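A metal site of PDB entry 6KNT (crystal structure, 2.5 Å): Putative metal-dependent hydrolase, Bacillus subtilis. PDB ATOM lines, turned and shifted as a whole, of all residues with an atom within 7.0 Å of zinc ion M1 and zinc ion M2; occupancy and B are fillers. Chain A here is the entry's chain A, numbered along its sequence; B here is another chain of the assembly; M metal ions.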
ATOM      1  N   TYR A  15     -23.719  18.102  16.791  1.00  0.00           N
ATOM      2  CA  TYR A  15     -23.595  18.364  15.358  1.00  0.00           C
ATOM      3  C   TYR A  15     -22.338  19.153  15.011  1.00  0.00           C
ATOM      4  O   TYR A  15     -21.909  20.026  15.796  1.00  0.00           O
ATOM      5  CB  TYR A  15     -24.831  19.093  14.840  1.00  0.00           C
ATOM      6  CG  TYR A  15     -25.912  18.128  14.455  1.00  0.00           C
ATOM      7  CD1 TYR A  15     -26.008  17.638  13.142  1.00  0.00           C
ATOM      8  CD2 TYR A  15     -26.823  17.648  15.413  1.00  0.00           C
ATOM      9  CE1 TYR A  15     -26.999  16.745  12.782  1.00  0.00           C
ATOM     10  CE2 TYR A  15     -27.786  16.738  15.078  1.00  0.00           C
ATOM     11  CZ  TYR A  15     -27.888  16.287  13.779  1.00  0.00           C
ATOM     12  OH  TYR A  15     -28.867  15.384  13.458  1.00  0.00           O
ATOM     13  N   GLY A  16     -21.753  18.850  13.851  1.00  0.00           N
ATOM     14  CA  GLY A  16     -20.675  19.636  13.298  1.00  0.00           C
ATOM     15  C   GLY A  16     -21.075  20.940  12.615  1.00  0.00           C
ATOM     16  O   GLY A  16     -22.078  21.023  11.872  1.00  0.00           O
ATOM     17  N   GLY A  17     -20.271  21.979  12.835  1.00  0.00           N
ATOM     18  CA  GLY A  17     -20.378  23.209  12.067  1.00  0.00           C
ATOM     19  C   GLY A  17     -21.476  24.109  12.594  1.00  0.00           C
ATOM     20  O   GLY A  17     -21.216  25.240  12.989  1.00  0.00           O
ATOM     21  N   SER A  26     -21.101  21.088  19.362  1.00  0.00           N
ATOM     22  CA  SER A  26     -20.288  20.446  20.399  1.00  0.00           C
ATOM     23  C   SER A  26     -20.456  20.989  21.806  1.00  0.00           C
ATOM     24  O   SER A  26     -20.159  22.163  22.071  1.00  0.00           O
ATOM     25  CB  SER A  26     -18.819  20.523  20.001  1.00  0.00           C
ATOM     26  OG  SER A  26     -18.582  19.752  18.839  1.00  0.00           O
ATOM     27  N   ASP A  40     -16.348  21.996  25.691  1.00  0.00           N
ATOM     28  CA  ASP A  40     -16.822  22.729  24.532  1.00  0.00           C
ATOM     29  C   ASP A  40     -18.228  23.338  24.753  1.00  0.00           C
ATOM     30  O   ASP A  40     -18.997  22.861  25.596  1.00  0.00           O
ATOM     31  CB  ASP A  40     -16.736  21.880  23.262  1.00  0.00           C
ATOM     32  CG  ASP A  40     -15.301  21.795  22.723  1.00  0.00           C
ATOM     33  OD1 ASP A  40     -14.412  22.542  23.247  1.00  0.00           O
ATOM     34  OD2 ASP A  40     -15.071  20.998  21.763  1.00  0.00           O
ATOM     35  N   SER A  64     -11.711  22.888  23.414  1.00  0.00           N
ATOM     36  CA  SER A  64     -10.698  22.221  22.616  1.00  0.00           C
ATOM     37  C   SER A  64     -10.042  23.181  21.626  1.00  0.00           C
ATOM     38  O   SER A  64      -8.846  23.072  21.331  1.00  0.00           O
ATOM     39  CB  SER A  64     -11.298  21.018  21.891  1.00  0.00           C
ATOM     40  OG  SER A  64     -12.236  21.426  20.927  1.00  0.00           O
ATOM     41  N   HIS A  65     -10.843  24.097  21.101  1.00  0.00           N
ATOM     42  CA  HIS A  65     -10.377  25.051  20.083  1.00  0.00           C
ATOM     43  C   HIS A  65     -11.410  26.150  19.839  1.00  0.00           C
ATOM     44  O   HIS A  65     -12.555  26.053  20.312  1.00  0.00           O
ATOM     45  CB  HIS A  65      -9.948  24.340  18.782  1.00  0.00           C
ATOM     46  CG  HIS A  65     -11.064  23.737  17.972  1.00  0.00           C
ATOM     47  ND1 HIS A  65     -11.879  22.723  18.448  1.00  0.00           N
ATOM     48  CD2 HIS A  65     -11.433  23.938  16.683  1.00  0.00           C
ATOM     49  CE1 HIS A  65     -12.724  22.355  17.498  1.00  0.00           C
ATOM     50  NE2 HIS A  65     -12.476  23.079  16.416  1.00  0.00           N
ATOM     51  N   TYR A  66     -11.035  27.175  19.093  1.00  0.00           N
ATOM     52  CA  TYR A  66     -11.874  28.352  19.010  1.00  0.00           C
ATOM     53  C   TYR A  66     -12.645  28.444  17.715  1.00  0.00           C
ATOM     54  O   TYR A  66     -12.760  29.514  17.149  1.00  0.00           O
ATOM     55  CB  TYR A  66     -11.049  29.611  19.255  1.00  0.00           C
ATOM     56  CG  TYR A  66     -10.356  29.616  20.590  1.00  0.00           C
ATOM     57  CD1 TYR A  66     -11.090  29.748  21.771  1.00  0.00           C
ATOM     58  CD2 TYR A  66      -8.976  29.461  20.681  1.00  0.00           C
ATOM     59  CE1 TYR A  66     -10.451  29.762  23.014  1.00  0.00           C
ATOM     60  CE2 TYR A  66      -8.340  29.456  21.916  1.00  0.00           C
ATOM     61  CZ  TYR A  66      -9.089  29.602  23.073  1.00  0.00           C
ATOM     62  OH  TYR A  66      -8.467  29.601  24.305  1.00  0.00           O
ATOM     63  N   HIS A  67     -13.185  27.326  17.241  1.00  0.00           N
ATOM     64  CA  HIS A  67     -14.096  27.396  16.100  1.00  0.00           C
ATOM     65  C   HIS A  67     -15.473  27.713  16.647  1.00  0.00           C
ATOM     66  O   HIS A  67     -15.808  27.284  17.759  1.00  0.00           O
ATOM     67  CB  HIS A  67     -14.096  26.082  15.313  1.00  0.00           C
ATOM     68  CG  HIS A  67     -13.138  26.066  14.151  1.00  0.00           C
ATOM     69  ND1 HIS A  67     -12.685  24.888  13.579  1.00  0.00           N
ATOM     70  CD2 HIS A  67     -12.530  27.065  13.481  1.00  0.00           C
ATOM     71  CE1 HIS A  67     -11.865  25.180  12.582  1.00  0.00           C
ATOM     72  NE2 HIS A  67     -11.757  26.494  12.506  1.00  0.00           N
ATOM     73  N   HIS A  68     -16.280  28.445  15.871  1.00  0.00           N
ATOM     74  CA  HIS A  68     -17.601  28.896  16.275  1.00  0.00           C
ATOM     75  C   HIS A  68     -18.443  27.800  16.891  1.00  0.00           C
ATOM     76  O   HIS A  68     -19.175  28.033  17.852  1.00  0.00           O
ATOM     77  CB  HIS A  68     -18.389  29.477  15.094  1.00  0.00           C
ATOM     78  CG  HIS A  68     -17.741  30.666  14.456  1.00  0.00           C
ATOM     79  ND1 HIS A  68     -17.265  31.741  15.171  1.00  0.00           N
ATOM     80  CD2 HIS A  68     -17.522  30.952  13.149  1.00  0.00           C
ATOM     81  CE1 HIS A  68     -16.777  32.636  14.343  1.00  0.00           C
ATOM     82  NE2 HIS A  68     -16.926  32.190  13.102  1.00  0.00           N
ATOM     83  N   ASP A  69     -18.411  26.616  16.293  1.00  0.00           N
ATOM     84  CA  ASP A  69     -19.254  25.547  16.754  1.00  0.00           C
ATOM     85  C   ASP A  69     -18.759  24.909  18.062  1.00  0.00           C
ATOM     86  O   ASP A  69     -19.422  24.049  18.598  1.00  0.00           O
ATOM     87  CB  ASP A  69     -19.519  24.519  15.655  1.00  0.00           C
ATOM     88  CG  ASP A  69     -18.215  23.968  14.991  1.00  0.00           C
ATOM     89  OD1 ASP A  69     -17.209  24.726  14.745  1.00  0.00           O
ATOM     90  OD2 ASP A  69     -18.252  22.734  14.723  1.00  0.00           O
ATOM     91  N   HIS A  70     -17.643  25.382  18.597  1.00  0.00           N
ATOM     92  CA  HIS A  70     -17.217  24.967  19.935  1.00  0.00           C
ATOM     93  C   HIS A  70     -17.259  26.091  20.981  1.00  0.00           C
ATOM     94  O   HIS A  70     -17.047  25.811  22.191  1.00  0.00           O
ATOM     95  CB  HIS A  70     -15.833  24.256  19.919  1.00  0.00           C
ATOM     96  CG  HIS A  70     -15.811  23.073  19.009  1.00  0.00           C
ATOM     97  ND1 HIS A  70     -15.778  21.769  19.464  1.00  0.00           N
ATOM     98  CD2 HIS A  70     -15.944  22.985  17.666  1.00  0.00           C
ATOM     99  CE1 HIS A  70     -15.846  20.934  18.446  1.00  0.00           C
ATOM    100  NE2 HIS A  70     -15.957  21.646  17.347  1.00  0.00           N
ATOM    101  N   HIS A 140      -6.038  19.855  12.381  1.00  0.00           N
ATOM    102  CA  HIS A 140      -7.265  20.611  12.138  1.00  0.00           C
ATOM    103  C   HIS A 140      -6.723  21.963  11.678  1.00  0.00           C
ATOM    104  O   HIS A 140      -5.549  22.243  11.930  1.00  0.00           O
ATOM    105  CB  HIS A 140      -8.068  20.735  13.437  1.00  0.00           C
ATOM    106  CG  HIS A 140      -9.510  21.127  13.274  1.00  0.00           C
ATOM    107  ND1 HIS A 140     -10.406  20.405  12.505  1.00  0.00           N
ATOM    108  CD2 HIS A 140     -10.240  22.132  13.827  1.00  0.00           C
ATOM    109  CE1 HIS A 140     -11.596  20.983  12.557  1.00  0.00           C
ATOM    110  NE2 HIS A 140     -11.527  22.027  13.366  1.00  0.00           N
ATOM    111  N   PRO A 141      -7.529  22.795  10.974  1.00  0.00           N
ATOM    112  CA  PRO A 141      -6.915  24.029  10.424  1.00  0.00           C
ATOM    113  C   PRO A 141      -6.618  25.109  11.467  1.00  0.00           C
ATOM    114  O   PRO A 141      -5.938  26.078  11.170  1.00  0.00           O
ATOM    115  CB  PRO A 141      -7.935  24.550   9.394  1.00  0.00           C
ATOM    116  CG  PRO A 141      -8.925  23.473   9.190  1.00  0.00           C
ATOM    117  CD  PRO A 141      -8.864  22.534  10.411  1.00  0.00           C
ATOM    118  N   VAL A 142      -7.160  24.965  12.680  1.00  0.00           N
ATOM    119  CA  VAL A 142      -6.735  25.812  13.809  1.00  0.00           C
ATOM    120  C   VAL A 142      -6.149  24.931  14.903  1.00  0.00           C
ATOM    121  O   VAL A 142      -6.415  23.712  14.962  1.00  0.00           O
ATOM    122  CB  VAL A 142      -7.895  26.726  14.331  1.00  0.00           C
ATOM    123  CG1 VAL A 142      -8.402  27.653  13.201  1.00  0.00           C
ATOM    124  CG2 VAL A 142      -9.062  25.893  14.926  1.00  0.00           C
ATOM    125  N   CYS A 144      -5.836  22.956  18.053  1.00  0.00           N
ATOM    126  CA  CYS A 144      -6.919  22.191  18.660  1.00  0.00           C
ATOM    127  C   CYS A 144      -6.358  20.996  19.452  1.00  0.00           C
ATOM    128  O   CYS A 144      -5.369  20.391  19.036  1.00  0.00           O
ATOM    129  CB  CYS A 144      -7.873  21.688  17.567  1.00  0.00           C
ATOM    130  SG  CYS A 144      -9.333  20.725  18.179  1.00  0.00           S
ATOM    131  N   TYR A 158     -11.863  12.297  24.308  1.00  0.00           N
ATOM    132  CA  TYR A 158     -12.597  13.101  23.369  1.00  0.00           C
ATOM    133  C   TYR A 158     -11.577  13.547  22.296  1.00  0.00           C
ATOM    134  O   TYR A 158     -10.519  14.117  22.647  1.00  0.00           O
ATOM    135  CB  TYR A 158     -13.160  14.289  24.111  1.00  0.00           C
ATOM    136  CG  TYR A 158     -13.765  15.390  23.251  1.00  0.00           C
ATOM    137  CD1 TYR A 158     -14.686  15.100  22.263  1.00  0.00           C
ATOM    138  CD2 TYR A 158     -13.425  16.743  23.475  1.00  0.00           C
ATOM    139  CE1 TYR A 158     -15.255  16.119  21.492  1.00  0.00           C
ATOM    140  CE2 TYR A 158     -14.003  17.764  22.750  1.00  0.00           C
ATOM    141  CZ  TYR A 158     -14.913  17.453  21.756  1.00  0.00           C
ATOM    142  OH  TYR A 158     -15.490  18.462  21.010  1.00  0.00           O
ATOM    143  N   ALA A 160     -11.937  15.778  20.108  1.00  0.00           N
ATOM    144  CA  ALA A 160     -12.214  17.107  19.558  1.00  0.00           C
ATOM    145  C   ALA A 160     -12.209  16.976  18.009  1.00  0.00           C
ATOM    146  O   ALA A 160     -12.620  15.930  17.468  1.00  0.00           O
ATOM    147  CB  ALA A 160     -11.180  18.146  20.069  1.00  0.00           C
ATOM    148  N   ASP A 161     -11.748  18.004  17.290  1.00  0.00           N
ATOM    149  CA  ASP A 161     -11.783  17.976  15.826  1.00  0.00           C
ATOM    150  C   ASP A 161     -10.422  17.603  15.283  1.00  0.00           C
ATOM    151  O   ASP A 161      -9.408  18.205  15.682  1.00  0.00           O
ATOM    152  CB  ASP A 161     -12.185  19.343  15.247  1.00  0.00           C
ATOM    153  CG  ASP A 161     -13.662  19.624  15.385  1.00  0.00           C
ATOM    154  OD1 ASP A 161     -14.352  18.986  16.202  1.00  0.00           O
ATOM    155  OD2 ASP A 161     -14.133  20.496  14.623  1.00  0.00           O
ATOM    156  N   SER A 162     -10.388  16.655  14.345  1.00  0.00           N
ATOM    157  CA  SER A 162      -9.134  16.238  13.752  1.00  0.00           C
ATOM    158  C   SER A 162      -9.305  15.387  12.499  1.00  0.00           C
ATOM    159  O   SER A 162     -10.305  14.679  12.347  1.00  0.00           O
ATOM    160  CB  SER A 162      -8.346  15.381  14.758  1.00  0.00           C
ATOM    161  OG  SER A 162      -7.028  15.102  14.272  1.00  0.00           O
ATOM    162  N   GLU A 181     -14.932  12.316  16.794  1.00  0.00           N
ATOM    163  CA  GLU A 181     -15.598  13.060  15.763  1.00  0.00           C
ATOM    164  C   GLU A 181     -15.721  12.112  14.580  1.00  0.00           C
ATOM    165  O   GLU A 181     -14.898  11.188  14.413  1.00  0.00           O
ATOM    166  CB  GLU A 181     -14.811  14.308  15.350  1.00  0.00           C
ATOM    167  CG  GLU A 181     -13.555  14.067  14.449  1.00  0.00           C
ATOM    168  CD  GLU A 181     -13.566  14.955  13.246  1.00  0.00           C
ATOM    169  OE1 GLU A 181     -14.062  14.513  12.188  1.00  0.00           O
ATOM    170  OE2 GLU A 181     -13.118  16.125  13.334  1.00  0.00           O
ATOM    171  N   ASN A 183     -17.258  13.391  11.176  1.00  0.00           N
ATOM    172  CA  ASN A 183     -17.922  14.289  10.248  1.00  0.00           C
ATOM    173  C   ASN A 183     -18.159  13.681   8.837  1.00  0.00           C
ATOM    174  O   ASN A 183     -18.987  14.187   8.073  1.00  0.00           O
ATOM    175  CB  ASN A 183     -17.183  15.631  10.160  1.00  0.00           C
ATOM    176  CG  ASN A 183     -18.130  16.822   9.995  1.00  0.00           C
ATOM    177  OD1 ASN A 183     -19.007  16.812   9.157  1.00  0.00           O
ATOM    178  ND2 ASN A 183     -17.924  17.874  10.802  1.00  0.00           N
ATOM    179  N   ALA A 193     -10.487  18.991   5.250  1.00  0.00           N
ATOM    180  CA  ALA A 193     -11.243  19.742   6.240  1.00  0.00           C
ATOM    181  C   ALA A 193     -10.733  19.540   7.689  1.00  0.00           C
ATOM    182  O   ALA A 193     -11.196  20.230   8.615  1.00  0.00           O
ATOM    183  CB  ALA A 193     -12.737  19.425   6.129  1.00  0.00           C
ATOM    184  N   GLY A 194      -9.789  18.625   7.886  1.00  0.00           N
ATOM    185  CA  GLY A 194      -9.337  18.288   9.240  1.00  0.00           C
ATOM    186  C   GLY A 194     -10.380  17.474  10.006  1.00  0.00           C
ATOM    187  O   GLY A 194     -10.719  17.824  11.155  1.00  0.00           O
ATOM    188  N   HIS A 195     -10.906  16.420   9.388  1.00  0.00           N
ATOM    189  CA  HIS A 195     -11.966  15.598   9.987  1.00  0.00           C
ATOM    190  C   HIS A 195     -11.733  14.111   9.690  1.00  0.00           C
ATOM    191  O   HIS A 195     -10.941  13.735   8.793  1.00  0.00           O
ATOM    192  CB  HIS A 195     -13.383  16.003   9.472  1.00  0.00           C
ATOM    193  CG  HIS A 195     -13.879  17.299  10.048  1.00  0.00           C
ATOM    194  ND1 HIS A 195     -13.869  17.563  11.402  1.00  0.00           N
ATOM    195  CD2 HIS A 195     -14.356  18.412   9.446  1.00  0.00           C
ATOM    196  CE1 HIS A 195     -14.355  18.782  11.610  1.00  0.00           C
ATOM    197  NE2 HIS A 195     -14.644  19.316  10.440  1.00  0.00           N
ATOM    198  N   HIS A 217     -19.843  14.998  16.322  1.00  0.00           N
ATOM    199  CA  HIS A 217     -19.565  16.030  15.311  1.00  0.00           C
ATOM    200  C   HIS A 217     -20.206  15.630  13.934  1.00  0.00           C
ATOM    201  O   HIS A 217     -19.561  15.678  12.864  1.00  0.00           O
ATOM    202  CB  HIS A 217     -18.057  16.235  15.174  1.00  0.00           C
ATOM    203  CG  HIS A 217     -17.647  17.621  14.791  1.00  0.00           C
ATOM    204  ND1 HIS A 217     -17.560  18.038  13.474  1.00  0.00           N
ATOM    205  CD2 HIS A 217     -17.287  18.679  15.544  1.00  0.00           C
ATOM    206  CE1 HIS A 217     -17.142  19.292  13.444  1.00  0.00           C
ATOM    207  NE2 HIS A 217     -16.959  19.704  14.696  1.00  0.00           N
ATOM    208  N   PHE B  79     -21.168  29.284   9.189  1.00  0.00           N
ATOM    209  CA  PHE B  79     -20.817  27.893   8.927  1.00  0.00           C
ATOM    210  C   PHE B  79     -21.949  27.110   8.244  1.00  0.00           C
ATOM    211  O   PHE B  79     -21.669  26.234   7.457  1.00  0.00           O
ATOM    212  CB  PHE B  79     -20.376  27.154  10.209  1.00  0.00           C
ATOM    213  CG  PHE B  79     -18.939  27.417  10.628  1.00  0.00           C
ATOM    214  CD1 PHE B  79     -18.084  28.180   9.833  1.00  0.00           C
ATOM    215  CD2 PHE B  79     -18.453  26.881  11.816  1.00  0.00           C
ATOM    216  CE1 PHE B  79     -16.759  28.405  10.235  1.00  0.00           C
ATOM    217  CE2 PHE B  79     -17.137  27.075  12.219  1.00  0.00           C
ATOM    218  CZ  PHE B  79     -16.280  27.846  11.428  1.00  0.00           C
HETATM  219 ZN    ZN M   1     -15.941  21.493  15.143  1.00  0.00          ZN
HETATM  220 ZN    ZN M   2     -13.266  22.778  14.266  1.00  0.00          ZN
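N of Gly 17 is in hydrogen-bond range of OD2 of Asp 69 (2.9 Å). O of Gly 194 lies within hydrogen-bond range of ND1 of His 140 (2.9 Å). A ring nitrogen (ND1) of His 217 is in hydrogen-bond range of the side-chain amide nitrogen (ND2) of Asn 183, 2.7 Å away. A ring nitrogen (ND1) of His 65 sits at hydrogen-bond distance from the side-chain sulfur (SG) of Cys 144 (3.2 Å). OG of Ser 64 sits at hydrogen-bond distance from ND1 of His 65 (2.8 Å). The backbone carbonyl oxygen (O) of Asp 161 sits at hydrogen-bond distance from the side-chain sulfur (SG) of Cys 144. O of Asp 69 sits at hydrogen-bond distance from N of Ser 26 (3.5 Å). A ring nitrogen (NE2) of His 217 lies close to the side-chain carboxylate (OD2) of Asp 69 (3.3 Å).
The nearest printed residue that does not touch zinc ion M1 is His 65 (4.02 Å).
Of the 27 residues printed, 4 come within 4 Å of zinc ion M2. Along chain A the residues within 4 Å of zinc ion M2 span positions 65 to 161.
Zinc ion M1 is bound by NE2 of His 217, OD2 of Asp 161 and NE2 of His 70. Slightly farther from zinc ion M1 lies OD2 of Asp 69 (2.7 Å).
Zinc ion M2 is bound by NE2 of His 140. Zinc ion M2 is bound by ND1 of His 67. NE2 of His 65 binds zinc ion M2 (2.3 Å). OD2 of Asp 161 binds zinc ion M2 (2.5 Å).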
